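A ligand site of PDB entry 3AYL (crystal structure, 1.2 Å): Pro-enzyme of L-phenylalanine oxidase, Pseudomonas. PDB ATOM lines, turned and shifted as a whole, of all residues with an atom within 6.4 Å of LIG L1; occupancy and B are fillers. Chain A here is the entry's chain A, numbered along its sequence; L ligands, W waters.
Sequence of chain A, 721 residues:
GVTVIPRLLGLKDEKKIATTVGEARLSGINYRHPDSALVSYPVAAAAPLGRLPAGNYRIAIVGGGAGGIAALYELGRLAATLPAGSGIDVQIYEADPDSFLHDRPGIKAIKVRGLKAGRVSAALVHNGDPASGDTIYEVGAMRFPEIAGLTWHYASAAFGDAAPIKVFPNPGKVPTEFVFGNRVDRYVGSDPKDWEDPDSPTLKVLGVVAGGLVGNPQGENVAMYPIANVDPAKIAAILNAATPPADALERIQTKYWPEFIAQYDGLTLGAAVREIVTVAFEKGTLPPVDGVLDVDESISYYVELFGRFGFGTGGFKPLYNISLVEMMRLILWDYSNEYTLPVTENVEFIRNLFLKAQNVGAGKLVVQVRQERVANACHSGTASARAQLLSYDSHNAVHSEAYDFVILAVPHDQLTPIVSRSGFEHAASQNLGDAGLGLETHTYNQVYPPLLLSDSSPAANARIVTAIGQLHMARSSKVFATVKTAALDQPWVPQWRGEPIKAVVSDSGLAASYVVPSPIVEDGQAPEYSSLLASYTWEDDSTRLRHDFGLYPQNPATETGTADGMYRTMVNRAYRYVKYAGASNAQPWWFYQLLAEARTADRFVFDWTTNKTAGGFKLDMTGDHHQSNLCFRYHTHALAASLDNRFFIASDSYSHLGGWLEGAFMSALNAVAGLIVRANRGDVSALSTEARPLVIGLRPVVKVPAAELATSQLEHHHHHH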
ATOM      1  N   MET A 142      -3.097  15.703 -20.420  1.00  0.00           N
ATOM      2  CA  MET A 142      -2.125  15.409 -21.463  1.00  0.00           C
ATOM      3  C   MET A 142      -0.890  14.679 -21.057  1.00  0.00           C
ATOM      4  O   MET A 142      -0.182  14.199 -21.954  1.00  0.00           O
ATOM      5  CB  MET A 142      -1.792  16.636 -22.301  1.00  0.00           C
ATOM      6  CG  MET A 142      -0.914  17.631 -21.551  1.00  0.00           C
ATOM      7  SD  MET A 142      -0.693  19.159 -22.503  1.00  0.00           S
ATOM      8  CE  MET A 142       0.526  19.995 -21.459  1.00  0.00           C
ATOM      9  N   ARG A 143      -0.499  14.667 -19.783  1.00  0.00           N
ATOM     10  CA  ARG A 143       0.807  14.125 -19.419  1.00  0.00           C
ATOM     11  C   ARG A 143       0.646  13.366 -18.086  1.00  0.00           C
ATOM     12  O   ARG A 143       0.031  13.853 -17.137  1.00  0.00           O
ATOM     13  CB  ARG A 143       1.843  15.261 -19.308  1.00  0.00           C
ATOM     14  CG  ARG A 143       1.526  16.398 -18.401  1.00  0.00           C
ATOM     15  CD  ARG A 143       2.415  17.586 -18.704  1.00  0.00           C
ATOM     16  NE  ARG A 143       2.101  18.725 -17.849  1.00  0.00           N
ATOM     17  CZ  ARG A 143       2.549  19.931 -18.079  1.00  0.00           C
ATOM     18  NH1 ARG A 143       3.475  20.149 -18.965  1.00  0.00           N
ATOM     19  NH2 ARG A 143       2.046  20.950 -17.407  1.00  0.00           N
ATOM     20  N   THR A 313       7.603  20.989 -15.144  1.00  0.00           N
ATOM     21  CA  THR A 313       6.411  21.193 -15.969  1.00  0.00           C
ATOM     22  C   THR A 313       6.108  22.696 -16.155  1.00  0.00           C
ATOM     23  O   THR A 313       4.984  23.066 -16.403  1.00  0.00           O
ATOM     24  CB  THR A 313       5.186  20.428 -15.448  1.00  0.00           C
ATOM     25  OG1 THR A 313       4.913  20.852 -14.115  1.00  0.00           O
ATOM     26  CG2 THR A 313       5.383  18.930 -15.540  1.00  0.00           C
ATOM     27  N   PHE A 316       6.002  27.227 -11.496  1.00  0.00           N
ATOM     28  CA  PHE A 316       5.022  27.109 -10.431  1.00  0.00           C
ATOM     29  C   PHE A 316       4.765  28.386  -9.684  1.00  0.00           C
ATOM     30  O   PHE A 316       3.952  28.407  -8.767  1.00  0.00           O
ATOM     31  CB  PHE A 316       5.319  25.953  -9.459  1.00  0.00           C
ATOM     32  CG  PHE A 316       4.771  24.616  -9.875  1.00  0.00           C
ATOM     33  CD1 PHE A 316       4.558  24.262 -11.178  1.00  0.00           C
ATOM     34  CD2 PHE A 316       4.482  23.669  -8.898  1.00  0.00           C
ATOM     35  CE1 PHE A 316       4.036  23.030 -11.538  1.00  0.00           C
ATOM     36  CE2 PHE A 316       3.960  22.437  -9.258  1.00  0.00           C
ATOM     37  CZ  PHE A 316       3.745  22.105 -10.572  1.00  0.00           C
ATOM     38  N   LEU A 319       1.253  28.884  -9.045  1.00  0.00           N
ATOM     39  CA  LEU A 319       0.826  27.922  -8.001  1.00  0.00           C
ATOM     40  C   LEU A 319       1.416  28.220  -6.660  1.00  0.00           C
ATOM     41  O   LEU A 319       1.278  27.428  -5.732  1.00  0.00           O
ATOM     42  CB  LEU A 319       1.134  26.480  -8.467  1.00  0.00           C
ATOM     43  CG  LEU A 319       0.716  26.089  -9.859  1.00  0.00           C
ATOM     44  CD1 LEU A 319       0.907  24.599 -10.090  1.00  0.00           C
ATOM     45  CD2 LEU A 319      -0.721  26.506 -10.166  1.00  0.00           C
ATOM     46  N   LEU A 330       3.236  16.148  -4.485  1.00  0.00           N
ATOM     47  CA  LEU A 330       3.793  16.041  -5.825  1.00  0.00           C
ATOM     48  C   LEU A 330       5.253  15.687  -5.833  1.00  0.00           C
ATOM     49  O   LEU A 330       5.730  14.908  -6.691  1.00  0.00           O
ATOM     50  CB  LEU A 330       3.528  17.332  -6.600  1.00  0.00           C
ATOM     51  CG  LEU A 330       2.048  17.710  -6.784  1.00  0.00           C
ATOM     52  CD1 LEU A 330       1.924  19.018  -7.561  1.00  0.00           C
ATOM     53  CD2 LEU A 330       1.282  16.580  -7.450  1.00  0.00           C
ATOM     54  N   TYR A 335       6.305  13.773  -9.538  1.00  0.00           N
ATOM     55  CA  TYR A 335       5.174  13.999 -10.468  1.00  0.00           C
ATOM     56  C   TYR A 335       5.616  14.397 -11.858  1.00  0.00           C
ATOM     57  O   TYR A 335       4.830  14.171 -12.776  1.00  0.00           O
ATOM     58  CB  TYR A 335       4.243  15.093  -9.884  1.00  0.00           C
ATOM     59  CG  TYR A 335       4.694  16.474 -10.288  1.00  0.00           C
ATOM     60  CD1 TYR A 335       4.152  17.059 -11.362  1.00  0.00           C
ATOM     61  CD2 TYR A 335       5.760  17.123  -9.693  1.00  0.00           C
ATOM     62  CE1 TYR A 335       4.632  18.272 -11.903  1.00  0.00           C
ATOM     63  CE2 TYR A 335       6.251  18.325 -10.205  1.00  0.00           C
ATOM     64  CZ  TYR A 335       5.692  18.853 -11.316  1.00  0.00           C
ATOM     65  OH  TYR A 335       6.242  20.015 -11.872  1.00  0.00           O
ATOM     66  N   GLU A 338       6.911  12.232 -16.718  1.00  0.00           N
ATOM     67  CA  GLU A 338       5.594  11.933 -17.346  1.00  0.00           C
ATOM     68  C   GLU A 338       5.672  11.385 -18.759  1.00  0.00           C
ATOM     69  O   GLU A 338       6.643  11.609 -19.514  1.00  0.00           O
ATOM     70  CB  GLU A 338       4.772  13.248 -17.362  1.00  0.00           C
ATOM     71  CG  GLU A 338       4.460  13.778 -15.976  1.00  0.00           C
ATOM     72  CD  GLU A 338       4.213  15.207 -15.883  1.00  0.00           C
ATOM     73  OE1 GLU A 338       4.233  15.939 -16.872  1.00  0.00           O
ATOM     74  OE2 GLU A 338       4.003  15.751 -14.716  1.00  0.00           O
ATOM     75  N   TYR A 536      -0.169  27.656 -22.133  1.00  0.00           N
ATOM     76  CA  TYR A 536      -0.887  26.837 -21.161  1.00  0.00           C
ATOM     77  C   TYR A 536      -0.670  27.527 -19.830  1.00  0.00           C
ATOM     78  O   TYR A 536       0.483  27.536 -19.319  1.00  0.00           O
ATOM     79  CB  TYR A 536      -0.350  25.398 -21.173  1.00  0.00           C
ATOM     80  CG  TYR A 536      -0.958  24.502 -20.126  1.00  0.00           C
ATOM     81  CD1 TYR A 536      -0.259  23.395 -19.695  1.00  0.00           C
ATOM     82  CD2 TYR A 536      -2.192  24.738 -19.541  1.00  0.00           C
ATOM     83  CE1 TYR A 536      -0.756  22.559 -18.733  1.00  0.00           C
ATOM     84  CE2 TYR A 536      -2.663  23.902 -18.519  1.00  0.00           C
ATOM     85  CZ  TYR A 536      -1.942  22.825 -18.115  1.00  0.00           C
ATOM     86  OH  TYR A 536      -2.444  22.083 -17.092  1.00  0.00           O
ATOM     87  N   TRP A 538      -1.970  28.745 -15.740  1.00  0.00           N
ATOM     88  CA  TRP A 538      -2.672  28.486 -14.489  1.00  0.00           C
ATOM     89  C   TRP A 538      -2.893  29.737 -13.700  1.00  0.00           C
ATOM     90  O   TRP A 538      -2.061  30.659 -13.731  1.00  0.00           O
ATOM     91  CB  TRP A 538      -1.789  27.583 -13.606  1.00  0.00           C
ATOM     92  CG  TRP A 538      -1.499  26.226 -14.192  1.00  0.00           C
ATOM     93  CD1 TRP A 538      -2.394  25.402 -14.764  1.00  0.00           C
ATOM     94  CD2 TRP A 538      -0.252  25.572 -14.246  1.00  0.00           C
ATOM     95  NE1 TRP A 538      -1.789  24.250 -15.174  1.00  0.00           N
ATOM     96  CE2 TRP A 538      -0.454  24.336 -14.898  1.00  0.00           C
ATOM     97  CE3 TRP A 538       1.050  25.914 -13.848  1.00  0.00           C
ATOM     98  CZ2 TRP A 538       0.608  23.445 -15.132  1.00  0.00           C
ATOM     99  CZ3 TRP A 538       2.076  25.018 -14.085  1.00  0.00           C
ATOM    100  CH2 TRP A 538       1.839  23.801 -14.704  1.00  0.00           C
ATOM    101  N   PHE A 617      -9.114  22.324 -12.239  1.00  0.00           N
ATOM    102  CA  PHE A 617      -8.889  21.190 -11.329  1.00  0.00           C
ATOM    103  C   PHE A 617      -8.592  21.757  -9.956  1.00  0.00           C
ATOM    104  O   PHE A 617      -8.086  22.859  -9.804  1.00  0.00           O
ATOM    105  CB  PHE A 617      -7.711  20.339 -11.786  1.00  0.00           C
ATOM    106  CG  PHE A 617      -6.503  21.113 -12.250  1.00  0.00           C
ATOM    107  CD1 PHE A 617      -5.628  21.622 -11.335  1.00  0.00           C
ATOM    108  CD2 PHE A 617      -6.288  21.414 -13.564  1.00  0.00           C
ATOM    109  CE1 PHE A 617      -4.601  22.448 -11.727  1.00  0.00           C
ATOM    110  CE2 PHE A 617      -5.260  22.277 -13.954  1.00  0.00           C
ATOM    111  CZ  PHE A 617      -4.428  22.794 -13.025  1.00  0.00           C
ATOM    112  N   LYS A 618      -8.863  20.942  -8.922  1.00  0.00           N
ATOM    113  CA  LYS A 618      -8.620  21.387  -7.562  1.00  0.00           C
ATOM    114  C   LYS A 618      -7.111  21.485  -7.258  1.00  0.00           C
ATOM    115  O   LYS A 618      -6.367  20.526  -7.485  1.00  0.00           O
ATOM    116  CB  LYS A 618      -9.249  20.410  -6.572  1.00  0.00           C
ATOM    117  CG  LYS A 618      -9.006  20.809  -5.121  1.00  0.00           C
ATOM    118  CD  LYS A 618      -9.665  19.867  -4.102  1.00  0.00           C
ATOM    119  CE  LYS A 618      -9.028  18.483  -4.008  1.00  0.00           C
ATOM    120  NZ  LYS A 618      -7.621  18.545  -3.439  1.00  0.00           N
ATOM    121  N   LEU A 619      -6.712  22.591  -6.580  1.00  0.00           N
ATOM    122  CA  LEU A 619      -5.433  22.655  -5.921  1.00  0.00           C
ATOM    123  C   LEU A 619      -5.660  23.303  -4.572  1.00  0.00           C
ATOM    124  O   LEU A 619      -6.320  24.343  -4.500  1.00  0.00           O
ATOM    125  CB  LEU A 619      -4.375  23.488  -6.704  1.00  0.00           C
ATOM    126  CG  LEU A 619      -3.771  22.814  -7.903  1.00  0.00           C
ATOM    127  CD1 LEU A 619      -2.861  23.857  -8.614  1.00  0.00           C
ATOM    128  CD2 LEU A 619      -2.940  21.572  -7.509  1.00  0.00           C
ATOM    129  N   GLY A 658      -5.827  16.493  -7.061  1.00  0.00           N
ATOM    130  CA  GLY A 658      -6.564  17.318  -8.007  1.00  0.00           C
ATOM    131  C   GLY A 658      -5.684  17.687  -9.192  1.00  0.00           C
ATOM    132  O   GLY A 658      -4.491  17.966  -9.017  1.00  0.00           O
ATOM    133  N   GLY A 659      -6.247  17.657 -10.390  1.00  0.00           N
ATOM    134  CA  GLY A 659      -5.444  17.896 -11.572  1.00  0.00           C
ATOM    135  C   GLY A 659      -4.756  16.714 -12.157  1.00  0.00           C
ATOM    136  O   GLY A 659      -3.963  16.873 -13.070  1.00  0.00           O
ATOM    137  N   TRP A 660      -5.112  15.520 -11.700  1.00  0.00           N
ATOM    138  CA  TRP A 660      -4.561  14.278 -12.261  1.00  0.00           C
ATOM    139  C   TRP A 660      -5.671  13.260 -12.424  1.00  0.00           C
ATOM    140  O   TRP A 660      -6.501  13.066 -11.491  1.00  0.00           O
ATOM    141  CB  TRP A 660      -3.471  13.674 -11.362  1.00  0.00           C
ATOM    142  CG  TRP A 660      -2.399  14.649 -11.069  1.00  0.00           C
ATOM    143  CD1 TRP A 660      -2.282  15.420  -9.985  1.00  0.00           C
ATOM    144  CD2 TRP A 660      -1.303  14.996 -11.911  1.00  0.00           C
ATOM    145  NE1 TRP A 660      -1.213  16.219 -10.056  1.00  0.00           N
ATOM    146  CE2 TRP A 660      -0.563  15.976 -11.228  1.00  0.00           C
ATOM    147  CE3 TRP A 660      -0.899  14.628 -13.165  1.00  0.00           C
ATOM    148  CZ2 TRP A 660       0.570  16.541 -11.766  1.00  0.00           C
ATOM    149  CZ3 TRP A 660       0.256  15.193 -13.725  1.00  0.00           C
ATOM    150  CH2 TRP A 660       0.943  16.133 -13.011  1.00  0.00           C
HETATM  151  N1  LIG L   1      -1.573  17.919 -13.724  1.00  0.00           N
HETATM  152  C1  LIG L   1      -1.759  19.110 -14.601  1.00  0.00           C
HETATM  153  C2  LIG L   1      -0.517  19.431 -15.424  1.00  0.00           C
HETATM  154  O1  LIG L   1      -0.581  20.357 -16.250  1.00  0.00           O
HETATM  155  C3  LIG L   1      -2.237  20.307 -13.818  1.00  0.00           C
HETATM  156  C4  LIG L   1      -1.233  20.963 -12.990  1.00  0.00           C
HETATM  157  S1  LIG L   1      -0.470  20.053 -11.646  1.00  0.00           S
HETATM  158  C5  LIG L   1      -1.843  19.772 -10.796  1.00  0.00           C
HETATM  159  O2  LIG L   1       0.495  18.712 -15.262  1.00  0.00           O
HETATM  160  P1  LG2 L   2     -14.730  15.699 -15.092  1.00  0.00           P
HETATM  161  O1  LG2 L   2     -13.696  15.335 -16.076  1.00  0.00           O
HETATM  162  O2  LG2 L   2     -14.982  17.147 -14.825  1.00  0.00           O
HETATM  163  O3  LG2 L   2     -16.050  14.927 -15.492  1.00  0.00           O
HETATM  164  C1  LG2 L   2     -17.355  15.236 -14.920  1.00  0.00           C
HETATM  165  C2  LG2 L   2     -18.364  14.886 -15.942  1.00  0.00           C
HETATM  166  O4  LG2 L   2     -19.653  15.177 -15.335  1.00  0.00           O
HETATM  167  C3  LG2 L   2     -18.295  15.733 -17.237  1.00  0.00           C
HETATM  168  O5  LG2 L   2     -18.330  14.923 -18.387  1.00  0.00           O
HETATM  169  C4  LG2 L   2     -19.506  16.651 -17.103  1.00  0.00           C
HETATM  170  O6  LG2 L   2     -20.069  17.097 -18.322  1.00  0.00           O
HETATM  171  C5  LG2 L   2     -20.469  15.879 -16.237  1.00  0.00           C
HETATM  172  N1  LG2 L   2     -21.398  16.675 -15.500  1.00  0.00           N
HETATM  173  C6  LG2 L   2     -21.068  17.705 -14.661  1.00  0.00           C
HETATM  174  N2  LG2 L   2     -22.106  18.175 -13.992  1.00  0.00           N
HETATM  175  C7  LG2 L   2     -23.191  17.413 -14.406  1.00  0.00           C
HETATM  176  C8  LG2 L   2     -24.548  17.447 -14.078  1.00  0.00           C
HETATM  177  N3  LG2 L   2     -25.053  18.337 -13.207  1.00  0.00           N
HETATM  178  N4  LG2 L   2     -25.334  16.518 -14.670  1.00  0.00           N
HETATM  179  C9  LG2 L   2     -24.802  15.683 -15.566  1.00  0.00           C
HETATM  180  N5  LG2 L   2     -23.539  15.589 -15.995  1.00  0.00           N
HETATM  181  C10 LG2 L   2     -22.765  16.477 -15.347  1.00  0.00           C
HETATM  182  N6  LG2 L   2      -4.695  14.954 -15.535  1.00  0.00           N
HETATM  183  C11 LG2 L   2      -3.603  14.169 -15.764  1.00  0.00           C
HETATM  184  O7  LG2 L   2      -3.478  13.029 -15.300  1.00  0.00           O
HETATM  185  N7  LG2 L   2      -2.606  14.714 -16.543  1.00  0.00           N
HETATM  186  C12 LG2 L   2      -2.623  16.016 -17.042  1.00  0.00           C
HETATM  187  O8  LG2 L   2      -1.749  16.365 -17.921  1.00  0.00           O
HETATM  188  C13 LG2 L   2      -3.670  16.785 -16.654  1.00  0.00           C
HETATM  189  N8  LG2 L   2      -3.707  18.116 -17.055  1.00  0.00           N
HETATM  190  C14 LG2 L   2      -4.918  18.798 -17.044  1.00  0.00           C
HETATM  191  C15 LG2 L   2      -5.029  20.047 -17.603  1.00  0.00           C
HETATM  192  C16 LG2 L   2      -6.241  20.744 -17.644  1.00  0.00           C
HETATM  193  C17 LG2 L   2      -6.260  22.144 -18.268  1.00  0.00           C
HETATM  194  C18 LG2 L   2      -7.379  20.111 -17.132  1.00  0.00           C
HETATM  195  C19 LG2 L   2      -8.723  20.742 -17.258  1.00  0.00           C
HETATM  196  C20 LG2 L   2      -7.233  18.865 -16.536  1.00  0.00           C
HETATM  197  C21 LG2 L   2      -6.022  18.182 -16.431  1.00  0.00           C
HETATM  198  N9  LG2 L   2      -5.859  16.956 -15.782  1.00  0.00           N
HETATM  199  C22 LG2 L   2      -4.715  16.218 -16.001  1.00  0.00           C
HETATM  200  C23 LG2 L   2      -6.858  16.446 -14.835  1.00  0.00           C
HETATM  201  C24 LG2 L   2      -7.839  15.482 -15.422  1.00  0.00           C
HETATM  202  O9  LG2 L   2      -8.331  15.996 -16.629  1.00  0.00           O
HETATM  203  C25 LG2 L   2      -8.964  15.258 -14.387  1.00  0.00           C
HETATM  204  O10 LG2 L   2      -8.423  14.849 -13.145  1.00  0.00           O
HETATM  205  C26 LG2 L   2     -10.030  14.256 -14.744  1.00  0.00           C
HETATM  206  O11 LG2 L   2     -10.296  14.303 -16.188  1.00  0.00           O
HETATM  207  C27 LG2 L   2     -11.322  14.649 -13.972  1.00  0.00           C
HETATM  208  O12 LG2 L   2     -12.291  13.631 -14.051  1.00  0.00           O
HETATM  209  P2  LG2 L   2     -13.574  13.766 -13.113  1.00  0.00           P
HETATM  210  O13 LG2 L   2     -14.413  12.585 -13.421  1.00  0.00           O
HETATM  211  O14 LG2 L   2     -13.169  14.122 -11.740  1.00  0.00           O
HETATM  212  O15 LG2 L   2     -14.319  15.104 -13.650  1.00  0.00           O
HETATM  213  O   HOH W   1       2.276  20.233 -13.659  1.00  0.00           O
HETATM  214  O   HOH W   2      -1.218  19.004 -18.657  1.00  0.00           O
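The side-chain carboxylate (OE1) of Glu 338 is in salt-bridge range of the guanidinium group (NE) of Arg 143. The side-chain hydroxyl of Tyr 536 sits at hydrogen-bond distance from the indole nitrogen of Trp 538.
O of Gly 659 sits at hydrogen-bond distance from N1 of LIG L1. The backbone NH (N) of Met 142 sits at hydrogen-bond distance from an oxygen (O8) of LG2 L2 (2.9 Å). The backbone NH (N) of Arg 143 sits at hydrogen-bond distance from an oxygen (O8) of LG2 L2, 2.8 Å away. The guanidinium group (NH2) of Arg 143 lies within salt-bridge range of an oxygen (O1) of LIG L1. The side-chain hydroxyl of Tyr 536 lies within hydrogen-bond range of an oxygen (O1) of LIG L1 (2.7 Å). The backbone carbonyl oxygen (O) of Trp 660 is in hydrogen-bond range of an oxygen (O10) of LG2 L2, 3.1 Å away. The backbone carbonyl oxygen of Arg 143 is in hydrogen-bond range of a nitrogen (N7) of LG2 L2, 2.8 Å away.
Water W2 lies within hydrogen-bond range of O8 of LG2 L2 (2.8 Å), O1 of LIG L1 (2.8 Å) and NE of Arg 143 (3.4 Å). Water W1 bridges the side-chain hydroxyl of Thr 313 and an oxygen (O2) of LIG L1.
CZ2 of Trp 538 touches O1 of LIG L1, at 3.5 Å. CZ of Phe 617 touches C3 of LIG L1, 3.4 Å away. Leu 619 touches LIG L1 (CD2 to C5, 3.9 Å). Gly 658 touches LIG L1. Trp 660 touches LIG L1 (CH2 to N1, 3.2 Å).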
